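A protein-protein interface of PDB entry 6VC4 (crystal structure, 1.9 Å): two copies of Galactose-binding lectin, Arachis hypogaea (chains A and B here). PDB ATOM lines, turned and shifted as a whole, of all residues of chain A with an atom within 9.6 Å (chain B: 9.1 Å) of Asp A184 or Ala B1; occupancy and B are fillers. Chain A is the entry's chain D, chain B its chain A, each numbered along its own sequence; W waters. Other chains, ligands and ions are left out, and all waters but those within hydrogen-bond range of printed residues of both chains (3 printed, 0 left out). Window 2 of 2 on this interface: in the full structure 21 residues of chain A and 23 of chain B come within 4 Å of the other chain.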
ATOM      1  N   PRO A 152      27.002   6.936  18.521  1.00  0.00           N
ATOM      2  CA  PRO A 152      26.696   5.531  18.202  1.00  0.00           C
ATOM      3  C   PRO A 152      25.764   4.930  19.253  1.00  0.00           C
ATOM      4  O   PRO A 152      25.830   5.250  20.435  1.00  0.00           O
ATOM      5  CB  PRO A 152      28.078   4.852  18.203  1.00  0.00           C
ATOM      6  CG  PRO A 152      29.048   5.950  17.987  1.00  0.00           C
ATOM      7  CD  PRO A 152      28.460   7.128  18.703  1.00  0.00           C
ATOM      8  N   TRP A 153      24.853   4.095  18.802  1.00  0.00           N
ATOM      9  CA  TRP A 153      23.847   3.475  19.646  1.00  0.00           C
ATOM     10  C   TRP A 153      23.539   2.105  19.017  1.00  0.00           C
ATOM     11  O   TRP A 153      24.142   1.761  17.987  1.00  0.00           O
ATOM     12  CB  TRP A 153      22.626   4.432  19.737  1.00  0.00           C
ATOM     13  CG  TRP A 153      21.411   3.901  20.444  1.00  0.00           C
ATOM     14  CD1 TRP A 153      21.303   3.568  21.762  1.00  0.00           C
ATOM     15  CD2 TRP A 153      20.118   3.672  19.865  1.00  0.00           C
ATOM     16  NE1 TRP A 153      20.043   3.091  22.026  1.00  0.00           N
ATOM     17  CE2 TRP A 153      19.298   3.130  20.877  1.00  0.00           C
ATOM     18  CE3 TRP A 153      19.593   3.813  18.573  1.00  0.00           C
ATOM     19  CZ2 TRP A 153      17.944   2.820  20.661  1.00  0.00           C
ATOM     20  CZ3 TRP A 153      18.261   3.465  18.348  1.00  0.00           C
ATOM     21  CH2 TRP A 153      17.453   2.983  19.385  1.00  0.00           C
ATOM     22  N   ASN A 154      22.728   1.282  19.681  1.00  0.00           N
ATOM     23  CA  ASN A 154      22.364  -0.030  19.164  1.00  0.00           C
ATOM     24  C   ASN A 154      20.905  -0.266  19.419  1.00  0.00           C
ATOM     25  O   ASN A 154      20.485  -0.272  20.582  1.00  0.00           O
ATOM     26  CB  ASN A 154      23.245  -1.147  19.792  1.00  0.00           C
ATOM     27  CG  ASN A 154      22.911  -2.566  19.363  1.00  0.00           C
ATOM     28  OD1 ASN A 154      23.023  -3.508  20.157  1.00  0.00           O
ATOM     29  ND2 ASN A 154      22.525  -2.773  18.099  1.00  0.00           N
ATOM     30  N   VAL A 160      12.599  -2.804  25.223  1.00  0.00           N
ATOM     31  CA  VAL A 160      11.948  -1.570  25.675  1.00  0.00           C
ATOM     32  C   VAL A 160      13.090  -0.600  26.018  1.00  0.00           C
ATOM     33  O   VAL A 160      13.997  -0.948  26.787  1.00  0.00           O
ATOM     34  CB  VAL A 160      10.937  -1.762  26.824  1.00  0.00           C
ATOM     35  CG1 VAL A 160      10.351  -0.415  27.279  1.00  0.00           C
ATOM     36  CG2 VAL A 160       9.809  -2.712  26.398  1.00  0.00           C
ATOM     37  N   VAL A 161      13.066   0.576  25.380  1.00  0.00           N
ATOM     38  CA  VAL A 161      14.072   1.649  25.513  1.00  0.00           C
ATOM     39  C   VAL A 161      13.420   2.834  26.260  1.00  0.00           C
ATOM     40  O   VAL A 161      12.306   3.211  25.936  1.00  0.00           O
ATOM     41  CB  VAL A 161      14.614   2.087  24.118  1.00  0.00           C
ATOM     42  CG1 VAL A 161      15.689   3.167  24.250  1.00  0.00           C
ATOM     43  CG2 VAL A 161      15.142   0.897  23.316  1.00  0.00           C
ATOM     44  N   LYS A 162      14.110   3.393  27.256  1.00  0.00           N
ATOM     45  CA  LYS A 162      13.651   4.545  28.040  1.00  0.00           C
ATOM     46  C   LYS A 162      14.507   5.760  27.686  1.00  0.00           C
ATOM     47  O   LYS A 162      15.725   5.653  27.584  1.00  0.00           O
ATOM     48  CB  LYS A 162      13.727   4.247  29.551  1.00  0.00           C
ATOM     49  CG  LYS A 162      12.760   3.187  30.063  1.00  0.00           C
ATOM     50  CD  LYS A 162      12.662   3.239  31.583  1.00  0.00           C
ATOM     51  CE  LYS A 162      13.653   2.370  32.335  1.00  0.00           C
ATOM     52  NZ  LYS A 162      13.680   2.710  33.780  1.00  0.00           N
ATOM     53  N   ALA A 177      19.328  11.354  27.512  1.00  0.00           N
ATOM     54  CA  ALA A 177      19.857  10.130  28.148  1.00  0.00           C
ATOM     55  C   ALA A 177      18.959   8.970  27.714  1.00  0.00           C
ATOM     56  O   ALA A 177      17.724   9.032  27.865  1.00  0.00           O
ATOM     57  CB  ALA A 177      19.907  10.263  29.664  1.00  0.00           C
ATOM     58  N   VAL A 178      19.565   7.956  27.074  1.00  0.00           N
ATOM     59  CA  VAL A 178      18.874   6.780  26.535  1.00  0.00           C
ATOM     60  C   VAL A 178      19.301   5.540  27.313  1.00  0.00           C
ATOM     61  O   VAL A 178      20.496   5.234  27.350  1.00  0.00           O
ATOM     62  CB  VAL A 178      19.161   6.623  25.013  1.00  0.00           C
ATOM     63  CG1 VAL A 178      18.321   5.501  24.407  1.00  0.00           C
ATOM     64  CG2 VAL A 178      18.917   7.928  24.256  1.00  0.00           C
ATOM     65  N   THR A 179      18.334   4.832  27.936  1.00  0.00           N
ATOM     66  CA  THR A 179      18.593   3.620  28.721  1.00  0.00           C
ATOM     67  C   THR A 179      18.216   2.394  27.909  1.00  0.00           C
ATOM     68  O   THR A 179      17.019   2.156  27.648  1.00  0.00           O
ATOM     69  CB  THR A 179      17.866   3.639  30.087  1.00  0.00           C
ATOM     70  OG1 THR A 179      18.219   4.833  30.779  1.00  0.00           O
ATOM     71  CG2 THR A 179      18.241   2.437  30.972  1.00  0.00           C
ATOM     72  N   ASN A 180      19.249   1.622  27.529  1.00  0.00           N
ATOM     73  CA  ASN A 180      19.187   0.380  26.771  1.00  0.00           C
ATOM     74  C   ASN A 180      18.768  -0.801  27.659  1.00  0.00           C
ATOM     75  O   ASN A 180      18.673  -0.673  28.888  1.00  0.00           O
ATOM     76  CB  ASN A 180      20.528   0.090  26.098  1.00  0.00           C
ATOM     77  CG  ASN A 180      20.932   1.127  25.089  1.00  0.00           C
ATOM     78  OD1 ASN A 180      20.319   1.247  24.030  1.00  0.00           O
ATOM     79  ND2 ASN A 180      21.975   1.913  25.404  1.00  0.00           N
ATOM     80  N   ASP A 181      18.474  -1.937  27.010  1.00  0.00           N
ATOM     81  CA  ASP A 181      18.059  -3.193  27.639  1.00  0.00           C
ATOM     82  C   ASP A 181      19.220  -3.820  28.428  1.00  0.00           C
ATOM     83  O   ASP A 181      18.997  -4.297  29.544  1.00  0.00           O
ATOM     84  CB  ASP A 181      17.537  -4.161  26.558  1.00  0.00           C
ATOM     85  CG  ASP A 181      17.247  -5.577  27.011  1.00  0.00           C
ATOM     86  OD1 ASP A 181      16.298  -5.762  27.809  1.00  0.00           O
ATOM     87  OD2 ASP A 181      17.921  -6.510  26.510  1.00  0.00           O
ATOM     88  N   ASN A 182      20.441  -3.755  27.873  1.00  0.00           N
ATOM     89  CA  ASN A 182      21.664  -4.278  28.548  1.00  0.00           C
ATOM     90  C   ASN A 182      22.035  -3.391  29.744  1.00  0.00           C
ATOM     91  O   ASN A 182      23.056  -3.664  30.373  1.00  0.00           O
ATOM     92  CB  ASN A 182      22.831  -4.514  27.593  1.00  0.00           C
ATOM     93  CG  ASN A 182      23.589  -3.276  27.181  1.00  0.00           C
ATOM     94  OD1 ASN A 182      23.241  -2.164  27.550  1.00  0.00           O
ATOM     95  ND2 ASN A 182      24.626  -3.463  26.396  1.00  0.00           N
ATOM     96  N   GLY A 183      21.224  -2.364  30.006  1.00  0.00           N
ATOM     97  CA  GLY A 183      21.347  -1.456  31.163  1.00  0.00           C
ATOM     98  C   GLY A 183      22.271  -0.263  30.961  1.00  0.00           C
ATOM     99  O   GLY A 183      22.202   0.653  31.760  1.00  0.00           O
ATOM    100  N   ASP A 184      23.041  -0.236  29.887  1.00  0.00           N
ATOM    101  CA  ASP A 184      23.966   0.893  29.610  1.00  0.00           C
ATOM    102  C   ASP A 184      23.163   2.163  29.251  1.00  0.00           C
ATOM    103  O   ASP A 184      22.072   2.037  28.752  1.00  0.00           O
ATOM    104  CB  ASP A 184      24.875   0.615  28.410  1.00  0.00           C
ATOM    105  CG  ASP A 184      25.956  -0.445  28.563  1.00  0.00           C
ATOM    106  OD1 ASP A 184      26.034  -1.051  29.622  1.00  0.00           O
ATOM    107  OD2 ASP A 184      26.699  -0.645  27.597  1.00  0.00           O
ATOM    108  N   ILE A 185      23.723   3.337  29.512  1.00  0.00           N
ATOM    109  CA  ILE A 185      23.103   4.626  29.095  1.00  0.00           C
ATOM    110  C   ILE A 185      23.953   5.244  27.988  1.00  0.00           C
ATOM    111  O   ILE A 185      25.180   5.135  28.030  1.00  0.00           O
ATOM    112  CB  ILE A 185      22.930   5.640  30.236  1.00  0.00           C
ATOM    113  CG1 ILE A 185      24.258   5.954  30.912  1.00  0.00           C
ATOM    114  CG2 ILE A 185      21.875   5.188  31.222  1.00  0.00           C
ATOM    115  CD1 ILE A 185      24.343   7.323  31.469  1.00  0.00           C
ATOM    116  N   THR A 186      23.272   5.862  27.043  1.00  0.00           N
ATOM    117  CA  THR A 186      23.864   6.594  25.912  1.00  0.00           C
ATOM    118  C   THR A 186      23.397   8.036  26.089  1.00  0.00           C
ATOM    119  O   THR A 186      22.227   8.220  26.311  1.00  0.00           O
ATOM    120  CB  THR A 186      23.359   5.996  24.597  1.00  0.00           C
ATOM    121  OG1 THR A 186      23.560   4.588  24.587  1.00  0.00           O
ATOM    122  CG2 THR A 186      23.964   6.625  23.365  1.00  0.00           C
ATOM    123  N   THR A 187      24.309   8.997  26.063  1.00  0.00           N
ATOM    124  CA  THR A 187      23.902  10.399  26.178  1.00  0.00           C
ATOM    125  C   THR A 187      24.365  11.181  24.971  1.00  0.00           C
ATOM    126  O   THR A 187      25.364  10.825  24.335  1.00  0.00           O
ATOM    127  CB  THR A 187      24.419  11.104  27.457  1.00  0.00           C
ATOM    128  OG1 THR A 187      25.844  11.208  27.402  1.00  0.00           O
ATOM    129  CG2 THR A 187      23.943  10.464  28.739  1.00  0.00           C
ATOM    130  N   ALA B   1      31.457  -1.844  27.495  1.00  0.00           N
ATOM    131  CA  ALA B   1      31.283  -0.666  28.340  1.00  0.00           C
ATOM    132  C   ALA B   1      31.107  -1.045  29.817  1.00  0.00           C
ATOM    133  O   ALA B   1      30.623  -2.126  30.138  1.00  0.00           O
ATOM    134  CB  ALA B   1      30.094   0.141  27.859  1.00  0.00           C
ATOM    135  N   GLU B   2      31.526  -0.140  30.683  1.00  0.00           N
ATOM    136  CA  GLU B   2      31.501  -0.344  32.149  1.00  0.00           C
ATOM    137  C   GLU B   2      30.325   0.449  32.724  1.00  0.00           C
ATOM    138  O   GLU B   2      30.363   1.658  32.654  1.00  0.00           O
ATOM    139  CB  GLU B   2      32.842   0.125  32.688  1.00  0.00           C
ATOM    140  CG  GLU B   2      32.954   0.173  34.188  1.00  0.00           C
ATOM    141  CD  GLU B   2      34.407   0.358  34.588  1.00  0.00           C
ATOM    142  OE1 GLU B   2      35.202  -0.504  34.242  1.00  0.00           O
ATOM    143  OE2 GLU B   2      34.732   1.365  35.182  1.00  0.00           O
ATOM    144  N   THR B   3      29.348  -0.256  33.272  1.00  0.00           N
ATOM    145  CA  THR B   3      28.138   0.403  33.790  1.00  0.00           C
ATOM    146  C   THR B   3      27.922   0.141  35.285  1.00  0.00           C
ATOM    147  O   THR B   3      28.049  -0.988  35.705  1.00  0.00           O
ATOM    148  CB  THR B   3      26.935   0.043  32.905  1.00  0.00           C
ATOM    149  OG1 THR B   3      25.697   0.476  33.462  1.00  0.00           O
ATOM    150  CG2 THR B   3      26.859  -1.445  32.697  1.00  0.00           C
ATOM    151  N   VAL B   4      27.633   1.201  36.033  1.00  0.00           N
ATOM    152  CA  VAL B   4      27.232   1.110  37.460  1.00  0.00           C
ATOM    153  C   VAL B   4      25.754   1.506  37.500  1.00  0.00           C
ATOM    154  O   VAL B   4      25.425   2.565  37.042  1.00  0.00           O
ATOM    155  CB  VAL B   4      28.072   1.996  38.393  1.00  0.00           C
ATOM    156  CG1 VAL B   4      27.595   1.852  39.823  1.00  0.00           C
ATOM    157  CG2 VAL B   4      29.547   1.678  38.300  1.00  0.00           C
ATOM    158  N   SER B   5      24.918   0.624  38.005  1.00  0.00           N
ATOM    159  CA  SER B   5      23.461   0.857  38.047  1.00  0.00           C
ATOM    160  C   SER B   5      22.889   0.455  39.408  1.00  0.00           C
ATOM    161  O   SER B   5      23.150  -0.660  39.831  1.00  0.00           O
ATOM    162  CB  SER B   5      22.816   0.064  36.942  1.00  0.00           C
ATOM    163  OG  SER B   5      21.582   0.614  36.600  1.00  0.00           O
ATOM    164  N   ARG B  53      34.207   4.630  38.874  1.00  0.00           N
ATOM    165  CA  ARG B  53      35.274   5.077  37.982  1.00  0.00           C
ATOM    166  C   ARG B  53      34.623   6.007  36.957  1.00  0.00           C
ATOM    167  O   ARG B  53      33.964   5.528  36.029  1.00  0.00           O
ATOM    168  CB  ARG B  53      35.974   3.849  37.353  1.00  0.00           C
ATOM    169  CG  ARG B  53      37.216   4.105  36.521  1.00  0.00           C
ATOM    170  CD  ARG B  53      37.660   2.725  36.078  1.00  0.00           C
ATOM    171  NE  ARG B  53      38.592   2.763  34.965  1.00  0.00           N
ATOM    172  CZ  ARG B  53      38.596   1.886  33.969  1.00  0.00           C
ATOM    173  NH1 ARG B  53      37.689   0.917  33.922  1.00  0.00           N
ATOM    174  NH2 ARG B  53      39.504   1.972  33.006  1.00  0.00           N
ATOM    175  N   ASN B  61      38.777   8.434  28.232  1.00  0.00           N
ATOM    176  CA  ASN B  61      37.310   8.441  28.234  1.00  0.00           C
ATOM    177  C   ASN B  61      36.728   8.856  29.572  1.00  0.00           C
ATOM    178  O   ASN B  61      37.246   8.492  30.625  1.00  0.00           O
ATOM    179  CB  ASN B  61      36.735   7.049  27.845  1.00  0.00           C
ATOM    180  CG  ASN B  61      37.033   6.612  26.427  1.00  0.00           C
ATOM    181  OD1 ASN B  61      36.885   5.449  26.085  1.00  0.00           O
ATOM    182  ND2 ASN B  61      37.450   7.522  25.556  1.00  0.00           N
ATOM    183  N   SER B  64      29.343   8.978  31.222  1.00  0.00           N
ATOM    184  CA  SER B  64      28.095   9.770  31.253  1.00  0.00           C
ATOM    185  C   SER B  64      27.236   9.189  32.386  1.00  0.00           C
ATOM    186  O   SER B  64      27.441   8.045  32.754  1.00  0.00           O
ATOM    187  CB  SER B  64      27.338   9.738  29.940  1.00  0.00           C
ATOM    188  OG  SER B  64      27.987  10.459  28.932  1.00  0.00           O
ATOM    189  N   PHE B  65      26.369   9.989  32.974  1.00  0.00           N
ATOM    190  CA  PHE B  65      25.458   9.399  33.974  1.00  0.00           C
ATOM    191  C   PHE B  65      24.063  10.024  33.911  1.00  0.00           C
ATOM    192  O   PHE B  65      23.906  11.142  33.466  1.00  0.00           O
ATOM    193  CB  PHE B  65      26.072   9.362  35.370  1.00  0.00           C
ATOM    194  CG  PHE B  65      26.298  10.698  36.019  1.00  0.00           C
ATOM    195  CD1 PHE B  65      25.255  11.408  36.567  1.00  0.00           C
ATOM    196  CD2 PHE B  65      27.563  11.239  36.109  1.00  0.00           C
ATOM    197  CE1 PHE B  65      25.459  12.626  37.185  1.00  0.00           C
ATOM    198  CE2 PHE B  65      27.759  12.466  36.713  1.00  0.00           C
ATOM    199  CZ  PHE B  65      26.709  13.161  37.231  1.00  0.00           C
ATOM    200  N   LEU B  66      23.091   9.215  34.300  1.00  0.00           N
ATOM    201  CA  LEU B  66      21.687   9.620  34.468  1.00  0.00           C
ATOM    202  C   LEU B  66      21.328   9.262  35.906  1.00  0.00           C
ATOM    203  O   LEU B  66      21.529   8.140  36.303  1.00  0.00           O
ATOM    204  CB  LEU B  66      20.781   8.886  33.487  1.00  0.00           C
ATOM    205  CG  LEU B  66      19.292   9.027  33.771  1.00  0.00           C
ATOM    206  CD1 LEU B  66      18.834  10.463  33.561  1.00  0.00           C
ATOM    207  CD2 LEU B  66      18.492   8.057  32.931  1.00  0.00           C
ATOM    208  N   THR B 226      22.593   5.509  37.043  1.00  0.00           N
ATOM    209  CA  THR B 226      23.247   4.713  35.992  1.00  0.00           C
ATOM    210  C   THR B 226      24.394   5.538  35.407  1.00  0.00           C
ATOM    211  O   THR B 226      24.145   6.644  34.993  1.00  0.00           O
ATOM    212  CB  THR B 226      22.296   4.221  34.897  1.00  0.00           C
ATOM    213  OG1 THR B 226      21.197   3.492  35.429  1.00  0.00           O
ATOM    214  CG2 THR B 226      23.019   3.386  33.868  1.00  0.00           C
ATOM    215  N   SER B 227      25.589   4.971  35.388  1.00  0.00           N
ATOM    216  CA  SER B 227      26.761   5.618  34.755  1.00  0.00           C
ATOM    217  C   SER B 227      27.340   4.624  33.755  1.00  0.00           C
ATOM    218  O   SER B 227      27.321   3.472  34.046  1.00  0.00           O
ATOM    219  CB  SER B 227      27.786   6.030  35.760  1.00  0.00           C
ATOM    220  OG  SER B 227      28.365   4.919  36.403  1.00  0.00           O
ATOM    221  N   THR B 228      27.756   5.087  32.598  1.00  0.00           N
ATOM    222  CA  THR B 228      28.390   4.198  31.606  1.00  0.00           C
ATOM    223  C   THR B 228      29.712   4.826  31.153  1.00  0.00           C
ATOM    224  O   THR B 228      29.708   5.995  30.810  1.00  0.00           O
ATOM    225  CB  THR B 228      27.417   3.842  30.484  1.00  0.00           C
ATOM    226  OG1 THR B 228      26.319   3.165  31.071  1.00  0.00           O
ATOM    227  CG2 THR B 228      28.022   2.985  29.402  1.00  0.00           C
ATOM    228  N   LEU B 229      30.783   4.040  31.178  1.00  0.00           N
ATOM    229  CA  LEU B 229      32.128   4.478  30.737  1.00  0.00           C
ATOM    230  C   LEU B 229      32.515   3.644  29.516  1.00  0.00           C
ATOM    231  O   LEU B 229      32.469   2.432  29.604  1.00  0.00           O
ATOM    232  CB  LEU B 229      33.119   4.275  31.883  1.00  0.00           C
ATOM    233  CG  LEU B 229      34.581   4.557  31.569  1.00  0.00           C
ATOM    234  CD1 LEU B 229      34.776   5.977  31.075  1.00  0.00           C
ATOM    235  CD2 LEU B 229      35.455   4.290  32.765  1.00  0.00           C
ATOM    236  N   ILE B 230      32.801   4.301  28.404  1.00  0.00           N
ATOM    237  CA  ILE B 230      33.233   3.580  27.209  1.00  0.00           C
ATOM    238  C   ILE B 230      34.635   2.979  27.472  1.00  0.00           C
ATOM    239  O   ILE B 230      35.577   3.717  27.760  1.00  0.00           O
ATOM    240  CB  ILE B 230      33.208   4.500  25.951  1.00  0.00           C
ATOM    241  CG1 ILE B 230      31.736   4.831  25.491  1.00  0.00           C
ATOM    242  CG2 ILE B 230      34.074   3.943  24.798  1.00  0.00           C
ATOM    243  CD1 ILE B 230      30.724   3.646  25.317  1.00  0.00           C
ATOM    244  N   THR B 231      34.739   1.640  27.439  1.00  0.00           N
ATOM    245  CA  THR B 231      36.010   0.928  27.614  1.00  0.00           C
ATOM    246  C   THR B 231      36.474   0.595  26.200  1.00  0.00           C
ATOM    247  O   THR B 231      35.789  -0.166  25.505  1.00  0.00           O
ATOM    248  CB  THR B 231      35.857  -0.298  28.551  1.00  0.00           C
ATOM    249  OG1 THR B 231      34.795  -1.139  28.089  1.00  0.00           O
ATOM    250  CG2 THR B 231      35.624   0.096  30.013  1.00  0.00           C
ATOM    251  N   THR B 232      37.543   1.254  25.725  1.00  0.00           N
ATOM    252  CA  THR B 232      38.034   1.075  24.357  1.00  0.00           C
ATOM    253  C   THR B 232      39.569   0.991  24.353  1.00  0.00           C
ATOM    254  O   THR B 232      40.135  -0.011  24.789  1.00  0.00           O
ATOM    255  CB  THR B 232      37.479   2.196  23.439  1.00  0.00           C
ATOM    256  OG1 THR B 232      37.585   1.804  22.070  1.00  0.00           O
ATOM    257  CG2 THR B 232      38.144   3.556  23.660  1.00  0.00           C
HETATM  258  O   HOH W   1      21.182  -0.530  34.228  1.00  0.00           O
HETATM  259  O   HOH W   2      28.720  11.666  25.748  1.00  0.00           O
HETATM  260  O   HOH W   3      27.999  -2.854  29.348  1.00  0.00           O
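OG1 of Thr B231 is in hydrogen-bond range of N of Ala B1 (3.5 Å).
The backbone carbonyl oxygen (O) of Ser B227 lies close to the side-chain hydroxyl (OG1) of Thr B3 (3.5 Å).
OG of Ser B5 lies within hydrogen-bond range of OG1 of Thr B226 (3.1 Å).
The backbone NH (N) of Leu B66 sits at hydrogen-bond distance from the backbone carbonyl oxygen (O) of Thr B226 (2.9 Å).
The side-chain amide nitrogen (ND2) of Asn A180 lies within hydrogen-bond range of the backbone carbonyl oxygen (O) of Asp A184 (3.4 Å).
N of Asp A184 sits at hydrogen-bond distance from OD1 of Asn A182, 3.0 Å away.
Of the printed residues of chain B, Asp A184 touches Ala B1 (3.5 Å), Thr B3 (3.2 Å) and Thr B228 (3.6 Å).
No residue of chain B comes within 4 Å of Asn A182.
Gly A183 touches just these residues of chain B: Thr B3 and Thr B226.
Printed residues of chain A within 4 Å of Thr B228: Asp A184 and Ile A185.
Printed residues of chain B within 4 Å of Thr A179: Leu B66 (3.9 Å).
Of the printed residues of chain B, Thr A187 touches Ser B64.
Thr B232 touches none of the printed residues of chain A.
The nearest printed residue of chain A that does not touch Leu B66 is Ala A177 (4.05 Å).
Of the 17 printed residues of chain B, 7 touch a printed residue of chain A.
Hydrophobic or aromatic side chains of chain B that line the printed part of chain A: Ala B1 and Leu B66.
Of the 17 printed residues of chain A, 5 touch a printed residue of chain B.
Hydrophobic or aromatic side chains of chain A that line the printed part of chain B: Ile A185.
Among the printed residues, no Asp or Glu carboxylate lies within 4 Å of a Lys or Arg side-chain nitrogen of the other chain.
Among the printed residues, pairs that only touch across the chains: Asp A184 with Thr B3 (3.2 Å), Ile A185 with Thr B226 (3.4 Å), Ile A185 with Ser B64 (3.4 Å), Ile A185 with Phe B65 (3.4 Å), Asp A184 with Ala B1 (3.5 Å), Gly A183 with Thr B226 (3.5 Å), Asp A184 with Thr B228 (3.6 Å), Ile A185 with Leu B66 (3.6 Å), Thr A179 with Leu B66 (3.9 Å) and Gly A183 with Thr B3 (3.9 Å).
The side-chain hydroxyl (OG) of Ser B64 sits at hydrogen-bond distance from the side-chain hydroxyl (OG1) of Thr A187 (2.7 Å).
The side-chain hydroxyl (OG1) of Thr B228 lies within hydrogen-bond range of the backbone NH (N) of Ile A185, 3.0 Å away.
No position is printed for both chains.
Of the 12 pairs that touch across the chains among the printed residues, none has its exchanged pair printed and touching as well.
Water W1 lies within hydrogen-bond range of OG of Ser B5 (2.7 Å) and O of Gly A183 (2.9 Å).
Water W3 lies within hydrogen-bond range of the side-chain carboxylate (OD1) of Asp A184 (2.7 Å) and the backbone carbonyl oxygen (O) of Ala B1 (2.8 Å).
Water W2 bridges OG1 of Thr A187 (3.3 Å) and OG of Ser B64 (3.5 Å).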
